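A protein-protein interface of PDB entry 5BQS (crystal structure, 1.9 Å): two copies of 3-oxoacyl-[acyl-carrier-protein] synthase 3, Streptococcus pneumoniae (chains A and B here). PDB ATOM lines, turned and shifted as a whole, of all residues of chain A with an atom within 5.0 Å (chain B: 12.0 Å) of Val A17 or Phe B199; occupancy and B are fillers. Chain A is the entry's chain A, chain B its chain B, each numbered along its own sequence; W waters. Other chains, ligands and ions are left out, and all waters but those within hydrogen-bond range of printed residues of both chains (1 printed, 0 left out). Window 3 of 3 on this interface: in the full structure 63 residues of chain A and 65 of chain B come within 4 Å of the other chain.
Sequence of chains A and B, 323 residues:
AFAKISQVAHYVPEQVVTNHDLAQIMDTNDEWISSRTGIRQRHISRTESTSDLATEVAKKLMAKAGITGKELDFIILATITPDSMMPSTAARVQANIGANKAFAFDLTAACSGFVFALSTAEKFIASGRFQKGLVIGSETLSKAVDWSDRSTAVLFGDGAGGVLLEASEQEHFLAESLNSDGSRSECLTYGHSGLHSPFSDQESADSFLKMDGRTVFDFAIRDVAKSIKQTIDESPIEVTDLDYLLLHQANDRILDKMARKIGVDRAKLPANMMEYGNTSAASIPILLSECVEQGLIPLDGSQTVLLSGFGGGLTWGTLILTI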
ATOM      1  N   GLN A  15      27.436  19.770 -22.572  1.00  0.00           N
ATOM      2  CA  GLN A  15      26.568  18.649 -22.219  1.00  0.00           C
ATOM      3  C   GLN A  15      26.503  17.593 -23.318  1.00  0.00           C
ATOM      4  O   GLN A  15      26.154  17.896 -24.470  1.00  0.00           O
ATOM      5  CB  GLN A  15      25.164  19.126 -21.804  1.00  0.00           C
ATOM      6  CG  GLN A  15      24.236  17.980 -21.400  1.00  0.00           C
ATOM      7  CD  GLN A  15      22.901  18.452 -20.910  1.00  0.00           C
ATOM      8  OE1 GLN A  15      22.480  18.117 -19.800  1.00  0.00           O
ATOM      9  NE2 GLN A  15      22.198  19.218 -21.726  1.00  0.00           N
ATOM     10  N   VAL A  16      26.878  16.367 -22.957  1.00  0.00           N
ATOM     11  CA  VAL A  16      26.860  15.217 -23.854  1.00  0.00           C
ATOM     12  C   VAL A  16      25.695  14.321 -23.434  1.00  0.00           C
ATOM     13  O   VAL A  16      25.560  14.000 -22.258  1.00  0.00           O
ATOM     14  CB  VAL A  16      28.213  14.445 -23.852  1.00  0.00           C
ATOM     15  CG1 VAL A  16      28.116  13.130 -24.627  1.00  0.00           C
ATOM     16  CG2 VAL A  16      29.344  15.311 -24.397  1.00  0.00           C
ATOM     17  N   VAL A  17      24.871  13.913 -24.403  1.00  0.00           N
ATOM     18  CA  VAL A  17      23.775  12.992 -24.163  1.00  0.00           C
ATOM     19  C   VAL A  17      24.075  11.711 -24.951  1.00  0.00           C
ATOM     20  O   VAL A  17      24.050  11.711 -26.175  1.00  0.00           O
ATOM     21  CB  VAL A  17      22.379  13.630 -24.447  1.00  0.00           C
ATOM     22  CG1 VAL A  17      21.271  12.608 -24.272  1.00  0.00           C
ATOM     23  CG2 VAL A  17      22.132  14.820 -23.524  1.00  0.00           C
ATOM     24  N   THR A  18      24.425  10.636 -24.245  1.00  0.00           N
ATOM     25  CA  THR A  18      24.737   9.358 -24.896  1.00  0.00           C
ATOM     26  C   THR A  18      23.437   8.647 -25.245  1.00  0.00           C
ATOM     27  O   THR A  18      22.384   9.009 -24.711  1.00  0.00           O
ATOM     28  CB  THR A  18      25.616   8.474 -23.987  1.00  0.00           C
ATOM     29  OG1 THR A  18      24.837   7.988 -22.899  1.00  0.00           O
ATOM     30  CG2 THR A  18      26.862   9.190 -23.479  1.00  0.00           C
ATOM     31  N   ASN A  19      23.512   7.602 -26.085  1.00  0.00           N
ATOM     32  CA  ASN A  19      22.359   6.766 -26.439  1.00  0.00           C
ATOM     33  C   ASN A  19      21.787   6.092 -25.190  1.00  0.00           C
ATOM     34  O   ASN A  19      20.580   5.856 -25.115  1.00  0.00           O
ATOM     35  CB  ASN A  19      22.760   5.710 -27.466  1.00  0.00           C
ATOM     36  CG  ASN A  19      23.050   6.239 -28.853  1.00  0.00           C
ATOM     37  OD1 ASN A  19      22.816   7.406 -29.182  1.00  0.00           O
ATOM     38  ND2 ASN A  19      23.549   5.375 -29.709  1.00  0.00           N
ATOM     39  N   ASP A  21      21.760   7.529 -22.120  1.00  0.00           N
ATOM     40  CA  ASP A  21      20.994   8.581 -21.431  1.00  0.00           C
ATOM     41  C   ASP A  21      19.596   8.698 -22.049  1.00  0.00           C
ATOM     42  O   ASP A  21      18.627   8.958 -21.333  1.00  0.00           O
ATOM     43  CB  ASP A  21      21.698   9.941 -21.549  1.00  0.00           C
ATOM     44  CG  ASP A  21      23.037  10.042 -20.843  1.00  0.00           C
ATOM     45  OD1 ASP A  21      23.184   9.442 -19.749  1.00  0.00           O
ATOM     46  OD2 ASP A  21      23.928  10.750 -21.360  1.00  0.00           O
ATOM     47  N   LEU A  22      19.501   8.517 -23.384  1.00  0.00           N
ATOM     48  CA  LEU A  22      18.235   8.553 -24.113  1.00  0.00           C
ATOM     49  C   LEU A  22      17.344   7.382 -23.741  1.00  0.00           C
ATOM     50  O   LEU A  22      16.141   7.573 -23.562  1.00  0.00           O
ATOM     51  CB  LEU A  22      18.456   8.617 -25.623  1.00  0.00           C
ATOM     52  CG  LEU A  22      18.990   9.948 -26.138  1.00  0.00           C
ATOM     53  CD1 LEU A  22      19.002   9.962 -27.641  1.00  0.00           C
ATOM     54  CD2 LEU A  22      18.145  11.123 -25.635  1.00  0.00           C
ATOM     55  N   GLN A  24      16.812   6.229 -21.036  1.00  0.00           N
ATOM     56  CA  GLN A  24      16.231   6.617 -19.736  1.00  0.00           C
ATOM     57  C   GLN A  24      14.932   7.458 -19.882  1.00  0.00           C
ATOM     58  O   GLN A  24      14.114   7.538 -18.963  1.00  0.00           O
ATOM     59  CB  GLN A  24      17.310   7.395 -18.947  1.00  0.00           C
ATOM     60  CG  GLN A  24      16.827   8.297 -17.812  1.00  0.00           C
ATOM     61  CD  GLN A  24      17.845   9.343 -17.448  1.00  0.00           C
ATOM     62  OE1 GLN A  24      17.733  10.516 -17.824  1.00  0.00           O
ATOM     63  NE2 GLN A  24      18.878   8.940 -16.726  1.00  0.00           N
ATOM     64  N   ILE A  25      14.757   8.092 -21.030  1.00  0.00           N
ATOM     65  CA  ILE A  25      13.591   8.940 -21.288  1.00  0.00           C
ATOM     66  C   ILE A  25      12.709   8.398 -22.421  1.00  0.00           C
ATOM     67  O   ILE A  25      11.648   8.962 -22.704  1.00  0.00           O
ATOM     68  CB  ILE A  25      13.981  10.433 -21.519  1.00  0.00           C
ATOM     69  CG1 ILE A  25      14.998  10.581 -22.661  1.00  0.00           C
ATOM     70  CG2 ILE A  25      14.486  11.077 -20.225  1.00  0.00           C
ATOM     71  CD1 ILE A  25      14.920  11.893 -23.413  1.00  0.00           C
ATOM     72  N   GLN A  41      26.383   9.173 -29.535  1.00  0.00           N
ATOM     73  CA  GLN A  41      26.083  10.267 -28.616  1.00  0.00           C
ATOM     74  C   GLN A  41      25.844  11.526 -29.440  1.00  0.00           C
ATOM     75  O   GLN A  41      26.098  11.535 -30.650  1.00  0.00           O
ATOM     76  CB  GLN A  41      27.274  10.496 -27.657  1.00  0.00           C
ATOM     77  CG  GLN A  41      28.599  10.766 -28.393  1.00  0.00           C
ATOM     78  CD  GLN A  41      29.585  11.536 -27.563  1.00  0.00           C
ATOM     79  OE1 GLN A  41      30.188  11.018 -26.644  1.00  0.00           O
ATOM     80  NE2 GLN A  41      29.795  12.794 -27.891  1.00  0.00           N
ATOM     81  N   ARG A  42      25.384  12.593 -28.776  1.00  0.00           N
ATOM     82  CA  ARG A  42      25.164  13.898 -29.395  1.00  0.00           C
ATOM     83  C   ARG A  42      25.261  14.955 -28.304  1.00  0.00           C
ATOM     84  O   ARG A  42      25.087  14.644 -27.118  1.00  0.00           O
ATOM     85  CB  ARG A  42      23.804  13.959 -30.141  1.00  0.00           C
ATOM     86  CG  ARG A  42      22.559  14.205 -29.264  1.00  0.00           C
ATOM     87  CD  ARG A  42      22.082  12.980 -28.509  1.00  0.00           C
ATOM     88  NE  ARG A  42      21.634  11.917 -29.413  1.00  0.00           N
ATOM     89  CZ  ARG A  42      21.902  10.629 -29.260  1.00  0.00           C
ATOM     90  NH1 ARG A  42      22.629  10.210 -28.227  1.00  0.00           N
ATOM     91  NH2 ARG A  42      21.418   9.741 -30.118  1.00  0.00           N
ATOM     92  N   HIS A  43      25.545  16.196 -28.691  1.00  0.00           N
ATOM     93  CA  HIS A  43      25.626  17.286 -27.725  1.00  0.00           C
ATOM     94  C   HIS A  43      24.279  17.975 -27.665  1.00  0.00           C
ATOM     95  O   HIS A  43      23.639  18.166 -28.703  1.00  0.00           O
ATOM     96  CB  HIS A  43      26.771  18.251 -28.069  1.00  0.00           C
ATOM     97  CG  HIS A  43      28.138  17.644 -27.894  1.00  0.00           C
ATOM     98  ND1 HIS A  43      28.982  18.048 -26.871  1.00  0.00           N
ATOM     99  CD2 HIS A  43      28.753  16.667 -28.607  1.00  0.00           C
ATOM    100  CE1 HIS A  43      30.085  17.331 -27.014  1.00  0.00           C
ATOM    101  NE2 HIS A  43      29.980  16.460 -28.015  1.00  0.00           N
ATOM    102  N   ILE A  44      23.790  18.231 -26.446  1.00  0.00           N
ATOM    103  CA  ILE A  44      22.498  18.884 -26.240  1.00  0.00           C
ATOM    104  C   ILE A  44      22.730  20.121 -25.405  1.00  0.00           C
ATOM    105  O   ILE A  44      23.293  20.041 -24.311  1.00  0.00           O
ATOM    106  CB  ILE A  44      21.412  17.940 -25.616  1.00  0.00           C
ATOM    107  CG1 ILE A  44      21.106  16.683 -26.527  1.00  0.00           C
ATOM    108  CG2 ILE A  44      20.125  18.714 -25.249  1.00  0.00           C
ATOM    109  CD1 ILE A  44      20.334  16.920 -27.871  1.00  0.00           C
ATOM    110  N   SER A  45      22.294  21.266 -25.921  1.00  0.00           N
ATOM    111  CA  SER A  45      22.443  22.530 -25.224  1.00  0.00           C
ATOM    112  C   SER A  45      21.594  22.592 -23.958  1.00  0.00           C
ATOM    113  O   SER A  45      20.432  22.196 -23.965  1.00  0.00           O
ATOM    114  CB  SER A  45      22.106  23.690 -26.152  1.00  0.00           C
ATOM    115  OG  SER A  45      22.439  24.890 -25.484  1.00  0.00           O
ATOM    116  N   ARG A  46      22.196  23.062 -22.869  1.00  0.00           N
ATOM    117  CA  ARG A  46      21.486  23.200 -21.612  1.00  0.00           C
ATOM    118  C   ARG A  46      20.988  24.639 -21.462  1.00  0.00           C
ATOM    119  O   ARG A  46      19.841  24.834 -21.083  1.00  0.00           O
ATOM    120  CB  ARG A  46      22.357  22.770 -20.412  1.00  0.00           C
ATOM    121  CG  ARG A  46      21.540  22.644 -19.123  1.00  0.00           C
ATOM    122  CD  ARG A  46      22.042  21.640 -18.121  1.00  0.00           C
ATOM    123  NE  ARG A  46      21.303  20.369 -18.162  1.00  0.00           N
ATOM    124  CZ  ARG A  46      20.061  20.180 -17.706  1.00  0.00           C
ATOM    125  NH1 ARG A  46      19.372  21.190 -17.190  1.00  0.00           N
ATOM    126  NH2 ARG A  46      19.493  18.988 -17.793  1.00  0.00           N
ATOM    127  N   TRP A 147      10.591  14.921 -28.496  1.00  0.00           N
ATOM    128  CA  TRP A 147      11.266  14.007 -27.564  1.00  0.00           C
ATOM    129  C   TRP A 147      10.439  12.782 -27.201  1.00  0.00           C
ATOM    130  O   TRP A 147      11.004  11.812 -26.681  1.00  0.00           O
ATOM    131  CB  TRP A 147      11.757  14.753 -26.330  1.00  0.00           C
ATOM    132  CG  TRP A 147      12.923  15.633 -26.679  1.00  0.00           C
ATOM    133  CD1 TRP A 147      12.896  16.973 -26.905  1.00  0.00           C
ATOM    134  CD2 TRP A 147      14.272  15.207 -26.942  1.00  0.00           C
ATOM    135  NE1 TRP A 147      14.151  17.420 -27.252  1.00  0.00           N
ATOM    136  CE2 TRP A 147      15.020  16.358 -27.261  1.00  0.00           C
ATOM    137  CE3 TRP A 147      14.930  13.965 -26.892  1.00  0.00           C
ATOM    138  CZ2 TRP A 147      16.397  16.304 -27.561  1.00  0.00           C
ATOM    139  CZ3 TRP A 147      16.290  13.912 -27.169  1.00  0.00           C
ATOM    140  CH2 TRP A 147      17.008  15.070 -27.506  1.00  0.00           C
ATOM    141  N   GLY B 194      12.886  29.518 -27.463  1.00  0.00           N
ATOM    142  CA  GLY B 194      13.693  29.060 -26.341  1.00  0.00           C
ATOM    143  C   GLY B 194      14.078  27.609 -26.432  1.00  0.00           C
ATOM    144  O   GLY B 194      13.497  26.853 -27.225  1.00  0.00           O
ATOM    145  N   LEU B 195      15.070  27.209 -25.622  1.00  0.00           N
ATOM    146  CA  LEU B 195      15.501  25.807 -25.576  1.00  0.00           C
ATOM    147  C   LEU B 195      14.350  24.971 -25.015  1.00  0.00           C
ATOM    148  O   LEU B 195      13.596  25.472 -24.183  1.00  0.00           O
ATOM    149  CB  LEU B 195      16.762  25.643 -24.716  1.00  0.00           C
ATOM    150  CG  LEU B 195      18.061  26.252 -25.254  1.00  0.00           C
ATOM    151  CD1 LEU B 195      19.148  26.167 -24.221  1.00  0.00           C
ATOM    152  CD2 LEU B 195      18.558  25.524 -26.513  1.00  0.00           C
ATOM    153  N   HIS B 196      14.172  23.734 -25.515  1.00  0.00           N
ATOM    154  CA  HIS B 196      13.084  22.862 -25.092  1.00  0.00           C
ATOM    155  C   HIS B 196      13.520  21.411 -25.210  1.00  0.00           C
ATOM    156  O   HIS B 196      13.424  20.819 -26.281  1.00  0.00           O
ATOM    157  CB  HIS B 196      11.817  23.151 -25.940  1.00  0.00           C
ATOM    158  CG  HIS B 196      10.675  22.206 -25.704  1.00  0.00           C
ATOM    159  ND1 HIS B 196      10.458  21.125 -26.535  1.00  0.00           N
ATOM    160  CD2 HIS B 196       9.716  22.222 -24.751  1.00  0.00           C
ATOM    161  CE1 HIS B 196       9.384  20.519 -26.062  1.00  0.00           C
ATOM    162  NE2 HIS B 196       8.905  21.146 -24.993  1.00  0.00           N
ATOM    163  N   SER B 197      14.031  20.845 -24.121  1.00  0.00           N
ATOM    164  CA  SER B 197      14.472  19.449 -24.121  1.00  0.00           C
ATOM    165  C   SER B 197      14.521  18.906 -22.714  1.00  0.00           C
ATOM    166  O   SER B 197      14.649  19.701 -21.767  1.00  0.00           O
ATOM    167  CB  SER B 197      15.817  19.273 -24.854  1.00  0.00           C
ATOM    168  OG  SER B 197      16.946  19.308 -23.996  1.00  0.00           O
ATOM    169  N   PRO B 198      14.475  17.562 -22.524  1.00  0.00           N
ATOM    170  CA  PRO B 198      14.567  17.021 -21.151  1.00  0.00           C
ATOM    171  C   PRO B 198      15.934  17.296 -20.511  1.00  0.00           C
ATOM    172  O   PRO B 198      16.125  17.019 -19.332  1.00  0.00           O
ATOM    173  CB  PRO B 198      14.339  15.514 -21.351  1.00  0.00           C
ATOM    174  CG  PRO B 198      13.690  15.391 -22.701  1.00  0.00           C
ATOM    175  CD  PRO B 198      14.324  16.476 -23.513  1.00  0.00           C
ATOM    176  N   PHE B 199      16.867  17.882 -21.298  1.00  0.00           N
ATOM    177  CA  PHE B 199      18.243  18.197 -20.908  1.00  0.00           C
ATOM    178  C   PHE B 199      18.532  19.704 -20.992  1.00  0.00           C
ATOM    179  O   PHE B 199      19.689  20.111 -20.893  1.00  0.00           O
ATOM    180  CB  PHE B 199      19.232  17.403 -21.797  1.00  0.00           C
ATOM    181  CG  PHE B 199      18.878  15.943 -21.966  1.00  0.00           C
ATOM    182  CD1 PHE B 199      19.120  15.025 -20.942  1.00  0.00           C
ATOM    183  CD2 PHE B 199      18.274  15.490 -23.129  1.00  0.00           C
ATOM    184  CE1 PHE B 199      18.768  13.675 -21.089  1.00  0.00           C
ATOM    185  CE2 PHE B 199      17.928  14.142 -23.278  1.00  0.00           C
ATOM    186  CZ  PHE B 199      18.180  13.243 -22.264  1.00  0.00           C
ATOM    187  N   SER B 200      17.486  20.528 -21.149  1.00  0.00           N
ATOM    188  CA  SER B 200      17.637  21.979 -21.285  1.00  0.00           C
ATOM    189  C   SER B 200      16.941  22.726 -20.170  1.00  0.00           C
ATOM    190  O   SER B 200      15.902  22.278 -19.678  1.00  0.00           O
ATOM    191  CB  SER B 200      17.117  22.459 -22.640  1.00  0.00           C
ATOM    192  OG  SER B 200      17.834  21.874 -23.711  1.00  0.00           O
ATOM    193  N   ASP B 201      17.501  23.874 -19.774  1.00  0.00           N
ATOM    194  CA  ASP B 201      16.872  24.674 -18.737  1.00  0.00           C
ATOM    195  C   ASP B 201      15.611  25.344 -19.251  1.00  0.00           C
ATOM    196  O   ASP B 201      15.598  25.861 -20.375  1.00  0.00           O
ATOM    197  CB  ASP B 201      17.859  25.668 -18.096  1.00  0.00           C
ATOM    198  CG  ASP B 201      18.838  24.995 -17.148  1.00  0.00           C
ATOM    199  OD1 ASP B 201      18.585  23.833 -16.753  1.00  0.00           O
ATOM    200  OD2 ASP B 201      19.851  25.624 -16.801  1.00  0.00           O
ATOM    201  N   GLN B 202      14.529  25.242 -18.453  1.00  0.00           N
ATOM    202  CA  GLN B 202      13.202  25.798 -18.729  1.00  0.00           C
ATOM    203  C   GLN B 202      13.349  27.263 -19.110  1.00  0.00           C
ATOM    204  O   GLN B 202      13.967  28.043 -18.381  1.00  0.00           O
ATOM    205  CB  GLN B 202      12.263  25.633 -17.516  1.00  0.00           C
ATOM    206  CG  GLN B 202      12.104  24.193 -17.008  1.00  0.00           C
ATOM    207  CD  GLN B 202      11.138  23.371 -17.827  1.00  0.00           C
ATOM    208  OE1 GLN B 202       9.920  23.562 -17.776  1.00  0.00           O
ATOM    209  NE2 GLN B 202      11.661  22.399 -18.559  1.00  0.00           N
ATOM    210  N   GLU B 203      12.869  27.596 -20.303  1.00  0.00           N
ATOM    211  CA  GLU B 203      12.960  28.925 -20.894  1.00  0.00           C
ATOM    212  C   GLU B 203      11.580  29.470 -21.188  1.00  0.00           C
ATOM    213  O   GLU B 203      10.722  28.733 -21.693  1.00  0.00           O
ATOM    214  CB  GLU B 203      13.742  28.837 -22.219  1.00  0.00           C
ATOM    215  CG  GLU B 203      15.237  29.058 -22.086  1.00  0.00           C
ATOM    216  CD  GLU B 203      15.854  29.774 -23.273  1.00  0.00           C
ATOM    217  OE1 GLU B 203      15.484  30.944 -23.528  1.00  0.00           O
ATOM    218  OE2 GLU B 203      16.727  29.171 -23.936  1.00  0.00           O
HETATM  219  O   HOH W   1      12.158  19.843 -28.474  1.00  0.00           O
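The backbone carbonyl oxygen (O) of Phe B199 lies within hydrogen-bond range of the side-chain amide nitrogen (NE2) of Gln A15 (2.8 Å). The backbone carbonyl oxygen (O) of Ser A45 lies within hydrogen-bond range of the side-chain hydroxyl (OG) of Ser B200, 2.6 Å away. The backbone carbonyl oxygen (O) of Phe B199 lies within hydrogen-bond range of the guanidinium group (NE) of Arg A46, at 3.2 Å. The side-chain carboxylate (OD1) of Asp B201 is in salt-bridge range of the guanidinium group (NH1) of Arg A46 (2.8 Å).
No position is printed for both chains.
Among the printed residues, merely in contact across the chains: Val A17 with Phe B199, Leu A22 with Phe B199, Ile A25 with Pro B198, Ile A25 with Phe B199, Ile A44 with Ser B197, Ile A44 with Phe B199, Ser A45 with Leu B195, Ser A45 with Phe B199, Arg A46 with Leu B195, Arg A46 with Ser B200, Trp A147 with His B196, Trp A147 with Ser B197 and Trp A147 with Pro B198.
Of the printed residues of chain B, Gln A15 touches Phe B199 (2.8 Å). No residue of chain B comes within 4 Å of Val A16. Val A17 touches just one residue of chain B: Phe B199 (3.7 Å). No residue of chain B comes within 4 Å of Asn A19. No residue of chain B comes within 4 Å of Asp A21. No residue of chain B comes within 4 Å of Gln A41. No residue of chain B comes within 4 Å of Arg A42. No residue of chain B comes within 4 Å of His A43. Ile A44 touches just these residues of chain B: Ser B197 and Phe B199. Ser A45 touches three residues of chain B. Printed residues of chain B within 4 Å of Trp A147: His B196, Ser B197 and Pro B198. Of the printed residues of chain A, Leu B195 touches Ser A45 and Arg A46. Of the printed residues of chain A, Pro B198 touches Ile A25 (3.8 Å) and Trp A147 (3.6 Å). Of the printed residues of chain A, Ser B200 touches Ser A45 and Arg A46. Printed residues of chain A within 4 Å of Asp B201: Arg A46. The nearest residue of chain B that does not touch Val A17 is Ser B197 (6.9 Å).
O of Ile A44 lies within hydrogen-bond range of NE2 of Gln A15 (2.9 Å). OE1 of Gln A15 is in hydrogen-bond range of NE of Arg A46. O of Arg A42 lies within hydrogen-bond range of N of Val A17 (2.8 Å). The backbone NH of Leu B195 sits at hydrogen-bond distance from the side-chain carboxylate of Glu B203. N of Phe B199 lies close to OG of Ser B197 (3.1 Å). The side-chain hydroxyl of Ser B197 lies within hydrogen-bond range of the side-chain hydroxyl of Ser B200 (2.7 Å).
Water W1 lies within hydrogen-bond range of the backbone carbonyl oxygen of His B196 (2.7 Å) and the indole nitrogen of Trp A147 (3.4 Å).
Of the 10 printed residues of chain B, 7 touch a printed residue of chain A. Hydrophobic or aromatic side chains of chain B that line the printed part of chain A: Leu B195, Pro B198 and Phe B199. Of the 16 printed residues of chain A, 8 touch a printed residue of chain B.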
